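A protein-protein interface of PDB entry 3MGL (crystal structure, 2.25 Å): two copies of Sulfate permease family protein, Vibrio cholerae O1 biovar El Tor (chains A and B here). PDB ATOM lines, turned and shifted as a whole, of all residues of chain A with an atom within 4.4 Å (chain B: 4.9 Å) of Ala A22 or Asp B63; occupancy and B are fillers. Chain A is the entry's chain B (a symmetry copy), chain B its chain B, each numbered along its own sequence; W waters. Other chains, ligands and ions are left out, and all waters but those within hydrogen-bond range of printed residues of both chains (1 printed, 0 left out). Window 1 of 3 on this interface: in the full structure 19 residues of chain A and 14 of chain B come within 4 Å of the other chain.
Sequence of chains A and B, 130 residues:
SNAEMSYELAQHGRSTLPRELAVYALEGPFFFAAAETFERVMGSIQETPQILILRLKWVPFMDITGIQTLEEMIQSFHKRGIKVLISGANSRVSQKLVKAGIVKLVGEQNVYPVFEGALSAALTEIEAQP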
ATOM      1  N   GLU A  20      22.678  15.595   2.411  1.00  0.00           N
ATOM      2  CA  GLU A  20      21.308  15.349   2.878  1.00  0.00           C
ATOM      3  C   GLU A  20      20.830  13.908   2.667  1.00  0.00           C
ATOM      4  O   GLU A  20      19.771  13.528   3.168  1.00  0.00           O
ATOM      5  CB  GLU A  20      20.321  16.310   2.206  1.00  0.00           C
ATOM      6  CG  GLU A  20      20.518  17.798   2.568  1.00  0.00           C
ATOM      7  CD  GLU A  20      21.465  18.505   1.620  1.00  0.00           C
ATOM      8  OE1 GLU A  20      22.198  17.819   0.869  1.00  0.00           O
ATOM      9  OE2 GLU A  20      21.468  19.758   1.608  1.00  0.00           O
ATOM     10  N   LEU A  21      21.597  13.120   1.921  1.00  0.00           N
ATOM     11  CA  LEU A  21      21.141  11.813   1.437  1.00  0.00           C
ATOM     12  C   LEU A  21      22.040  10.681   1.903  1.00  0.00           C
ATOM     13  O   LEU A  21      23.244  10.723   1.692  1.00  0.00           O
ATOM     14  CB  LEU A  21      21.066  11.790  -0.100  1.00  0.00           C
ATOM     15  CG  LEU A  21      20.579  10.468  -0.764  1.00  0.00           C
ATOM     16  CD1 LEU A  21      19.246   9.928  -0.169  1.00  0.00           C
ATOM     17  CD2 LEU A  21      20.447  10.643  -2.269  1.00  0.00           C
ATOM     18  N   ALA A  22      21.436   9.666   2.509  1.00  0.00           N
ATOM     19  CA  ALA A  22      22.152   8.454   2.898  1.00  0.00           C
ATOM     20  C   ALA A  22      21.519   7.210   2.247  1.00  0.00           C
ATOM     21  O   ALA A  22      20.360   7.211   1.862  1.00  0.00           O
ATOM     22  CB  ALA A  22      22.197   8.317   4.408  1.00  0.00           C
ATOM     23  N   VAL A  23      22.316   6.167   2.087  1.00  0.00           N
ATOM     24  CA  VAL A  23      21.866   4.956   1.414  1.00  0.00           C
ATOM     25  C   VAL A  23      22.343   3.805   2.255  1.00  0.00           C
ATOM     26  O   VAL A  23      23.501   3.772   2.663  1.00  0.00           O
ATOM     27  CB  VAL A  23      22.463   4.846   0.003  1.00  0.00           C
ATOM     28  CG1 VAL A  23      22.018   3.540  -0.688  1.00  0.00           C
ATOM     29  CG2 VAL A  23      22.042   6.051  -0.831  1.00  0.00           C
ATOM     30  N   TYR A  24      21.448   2.866   2.524  1.00  0.00           N
ATOM     31  CA  TYR A  24      21.816   1.678   3.277  1.00  0.00           C
ATOM     32  C   TYR A  24      21.174   0.448   2.664  1.00  0.00           C
ATOM     33  O   TYR A  24      20.014   0.485   2.277  1.00  0.00           O
ATOM     34  CB  TYR A  24      21.421   1.809   4.750  1.00  0.00           C
ATOM     35  CG  TYR A  24      21.865   0.616   5.580  1.00  0.00           C
ATOM     36  CD1 TYR A  24      23.229   0.369   5.811  1.00  0.00           C
ATOM     37  CD2 TYR A  24      20.936  -0.259   6.144  1.00  0.00           C
ATOM     38  CE1 TYR A  24      23.647  -0.703   6.557  1.00  0.00           C
ATOM     39  CE2 TYR A  24      21.356  -1.353   6.915  1.00  0.00           C
ATOM     40  CZ  TYR A  24      22.702  -1.561   7.107  1.00  0.00           C
ATOM     41  OH  TYR A  24      23.122  -2.640   7.860  1.00  0.00           O
ATOM     42  N   PRO A  49      21.022  12.633   8.038  1.00  0.00           N
ATOM     43  CA  PRO A  49      20.589  13.018   6.689  1.00  0.00           C
ATOM     44  C   PRO A  49      19.103  13.366   6.680  1.00  0.00           C
ATOM     45  O   PRO A  49      18.392  12.982   7.592  1.00  0.00           O
ATOM     46  CB  PRO A  49      20.829  11.742   5.871  1.00  0.00           C
ATOM     47  CG  PRO A  49      20.658  10.639   6.855  1.00  0.00           C
ATOM     48  CD  PRO A  49      21.268  11.180   8.140  1.00  0.00           C
ATOM     49  N   ILE A  51      17.196  12.347   4.078  1.00  0.00           N
ATOM     50  CA  ILE A  51      16.558  11.201   3.415  1.00  0.00           C
ATOM     51  C   ILE A  51      17.461   9.978   3.473  1.00  0.00           C
ATOM     52  O   ILE A  51      18.652  10.042   3.173  1.00  0.00           O
ATOM     53  CB  ILE A  51      16.186  11.531   1.937  1.00  0.00           C
ATOM     54  CG1 ILE A  51      15.288  12.780   1.860  1.00  0.00           C
ATOM     55  CG2 ILE A  51      15.523  10.322   1.254  1.00  0.00           C
ATOM     56  CD1 ILE A  51      14.968  13.263   0.434  1.00  0.00           C
ATOM     57  N   LEU A  52      16.881   8.860   3.863  1.00  0.00           N
ATOM     58  CA  LEU A  52      17.589   7.601   3.816  1.00  0.00           C
ATOM     59  C   LEU A  52      16.894   6.663   2.832  1.00  0.00           C
ATOM     60  O   LEU A  52      15.670   6.509   2.870  1.00  0.00           O
ATOM     61  CB  LEU A  52      17.667   6.984   5.217  1.00  0.00           C
ATOM     62  CG  LEU A  52      18.270   5.573   5.272  1.00  0.00           C
ATOM     63  CD1 LEU A  52      19.771   5.590   5.210  1.00  0.00           C
ATOM     64  CD2 LEU A  52      17.832   4.918   6.541  1.00  0.00           C
ATOM     65  N   ILE A  53      17.673   6.047   1.946  1.00  0.00           N
ATOM     66  CA  ILE A  53      17.130   5.030   1.058  1.00  0.00           C
ATOM     67  C   ILE A  53      17.585   3.673   1.588  1.00  0.00           C
ATOM     68  O   ILE A  53      18.781   3.425   1.769  1.00  0.00           O
ATOM     69  CB  ILE A  53      17.570   5.221  -0.424  1.00  0.00           C
ATOM     70  CG1 ILE A  53      17.066   6.557  -0.963  1.00  0.00           C
ATOM     71  CG2 ILE A  53      17.043   4.075  -1.304  1.00  0.00           C
ATOM     72  CD1 ILE A  53      17.719   6.971  -2.283  1.00  0.00           C
ATOM     73  N   PHE B  61      31.128   4.420  -1.949  1.00  0.00           N
ATOM     74  CA  PHE B  61      30.606   5.768  -1.706  1.00  0.00           C
ATOM     75  C   PHE B  61      30.585   5.957  -0.197  1.00  0.00           C
ATOM     76  O   PHE B  61      30.766   4.998   0.550  1.00  0.00           O
ATOM     77  CB  PHE B  61      29.192   5.945  -2.280  1.00  0.00           C
ATOM     78  CG  PHE B  61      28.154   5.086  -1.599  1.00  0.00           C
ATOM     79  CD1 PHE B  61      27.492   5.536  -0.450  1.00  0.00           C
ATOM     80  CD2 PHE B  61      27.860   3.822  -2.089  1.00  0.00           C
ATOM     81  CE1 PHE B  61      26.538   4.734   0.200  1.00  0.00           C
ATOM     82  CE2 PHE B  61      26.905   3.004  -1.459  1.00  0.00           C
ATOM     83  CZ  PHE B  61      26.244   3.465  -0.308  1.00  0.00           C
ATOM     84  N   MET B  62      30.368   7.193   0.241  1.00  0.00           N
ATOM     85  CA  MET B  62      30.256   7.516   1.652  1.00  0.00           C
ATOM     86  C   MET B  62      29.171   8.566   1.840  1.00  0.00           C
ATOM     87  O   MET B  62      29.145   9.585   1.142  1.00  0.00           O
ATOM     88  CB  MET B  62      31.578   8.023   2.218  1.00  0.00           C
ATOM     89  CG  MET B  62      32.576   6.916   2.497  1.00  0.00           C
ATOM     90  SD  MET B  62      34.159   7.472   3.500  1.00  0.00           S
ATOM     91  CE  MET B  62      33.316   7.847   5.156  1.00  0.00           C
ATOM     92  N   ASP B  63      28.248   8.309   2.752  1.00  0.00           N
ATOM     93  CA  ASP B  63      27.312   9.346   3.118  1.00  0.00           C
ATOM     94  C   ASP B  63      27.733   9.898   4.463  1.00  0.00           C
ATOM     95  O   ASP B  63      28.771   9.497   5.010  1.00  0.00           O
ATOM     96  CB  ASP B  63      25.861   8.843   3.110  1.00  0.00           C
ATOM     97  CG  ASP B  63      25.648   7.663   4.029  1.00  0.00           C
ATOM     98  OD1 ASP B  63      26.184   7.695   5.162  1.00  0.00           O
ATOM     99  OD2 ASP B  63      24.955   6.692   3.608  1.00  0.00           O
ATOM    100  N   ILE B  64      26.926  10.812   4.983  1.00  0.00           N
ATOM    101  CA  ILE B  64      27.223  11.494   6.225  1.00  0.00           C
ATOM    102  C   ILE B  64      27.365  10.535   7.412  1.00  0.00           C
ATOM    103  O   ILE B  64      28.041  10.852   8.374  1.00  0.00           O
ATOM    104  CB  ILE B  64      26.170  12.600   6.506  1.00  0.00           C
ATOM    105  CG1 ILE B  64      26.602  13.495   7.673  1.00  0.00           C
ATOM    106  CG2 ILE B  64      24.778  11.992   6.733  1.00  0.00           C
ATOM    107  CD1 ILE B  64      25.603  14.619   7.955  1.00  0.00           C
ATOM    108  N   THR B  65      26.736   9.366   7.337  1.00  0.00           N
ATOM    109  CA  THR B  65      26.867   8.366   8.392  1.00  0.00           C
ATOM    110  C   THR B  65      28.263   7.736   8.368  1.00  0.00           C
ATOM    111  O   THR B  65      28.902   7.595   9.414  1.00  0.00           O
ATOM    112  CB  THR B  65      25.760   7.263   8.339  1.00  0.00           C
ATOM    113  OG1 THR B  65      25.898   6.488   7.139  1.00  0.00           O
ATOM    114  CG2 THR B  65      24.372   7.862   8.401  1.00  0.00           C
ATOM    115  N   GLY B  66      28.755   7.386   7.179  1.00  0.00           N
ATOM    116  CA  GLY B  66      30.123   6.869   7.050  1.00  0.00           C
ATOM    117  C   GLY B  66      31.159   7.914   7.426  1.00  0.00           C
ATOM    118  O   GLY B  66      32.159   7.613   8.077  1.00  0.00           O
ATOM    119  N   ILE B  67      30.922   9.149   7.001  1.00  0.00           N
ATOM    120  CA  ILE B  67      31.837  10.259   7.246  1.00  0.00           C
ATOM    121  C   ILE B  67      32.026  10.483   8.754  1.00  0.00           C
ATOM    122  O   ILE B  67      33.160  10.565   9.234  1.00  0.00           O
ATOM    123  CB  ILE B  67      31.321  11.564   6.582  1.00  0.00           C
ATOM    124  CG1 ILE B  67      31.509  11.522   5.057  1.00  0.00           C
ATOM    125  CG2 ILE B  67      31.958  12.828   7.212  1.00  0.00           C
ATOM    126  CD1 ILE B  67      32.958  11.390   4.557  1.00  0.00           C
ATOM    127  N   LYS B  96      34.674  13.415  -1.614  1.00  0.00           N
ATOM    128  CA  LYS B  96      33.915  13.441  -0.358  1.00  0.00           C
ATOM    129  C   LYS B  96      34.813  13.647   0.879  1.00  0.00           C
ATOM    130  O   LYS B  96      34.464  14.391   1.779  1.00  0.00           O
ATOM    131  CB  LYS B  96      33.113  12.139  -0.199  1.00  0.00           C
ATOM    132  CG  LYS B  96      31.854  12.277   0.634  1.00  0.00           C
ATOM    133  CD  LYS B  96      30.896  13.242  -0.027  1.00  0.00           C
ATOM    134  CE  LYS B  96      29.529  13.121   0.532  1.00  0.00           C
ATOM    135  NZ  LYS B  96      28.859  11.975  -0.113  1.00  0.00           N
HETATM  136  O   HOH W   1      24.897  11.970   3.377  1.00  0.00           O
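The side-chain carboxylate (OD2) of Asp B63 is in hydrogen-bond range of the backbone NH (N) of Val A23 (3.1 Å).
The side-chain carboxylate (OD1) of Asp B63 is in hydrogen-bond range of the backbone NH (N) of Thr B65 (2.8 Å).
The side-chain carboxylate (OD1) of Asp B63 sits at hydrogen-bond distance from the backbone NH (N) of Gly B66 (3.3 Å).
The backbone NH of Ala A22 sits at hydrogen-bond distance from the backbone carbonyl oxygen of Ile A51.
The backbone carbonyl oxygen (O) of Ala A22 lies within hydrogen-bond range of the backbone NH (N) of Ile A53, 2.9 Å away.
Among the printed residues, pairs that only touch across the chains: Ala A22 with Asp B63, Leu A21 with Asp B63 and Pro A49 with Ile B64.
Ala A22 touches one residue of chain B.
Of the printed residues of chain B, Pro A49 touches Ile B64 (3.9 Å).
Printed residues of chain B within 4 Å of Val A23: Asp B63.
Of the printed residues of chain B, Leu A21 touches Asp B63 (3.5 Å).
The nearest residue of chain B that does not touch Ala A22 is Thr B65 (4.6 Å).
Of the 8 printed residues of chain B, 2 touch a printed residue of chain A.
Printed residues of chain B that touch a printed residue of chain A: Asp B63 and Ile B64.
Hydrophobic or aromatic side chains of chain B that line the printed part of chain A: Ile B64.
No position is printed for both chains.
Of the 4 pairs that touch across the chains among the printed residues, none has its exchanged pair printed and touching as well.
Water W1 bridges the backbone carbonyl oxygen of Leu A21 (2.7 Å) and the backbone NH of Ile B64 (2.8 Å).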
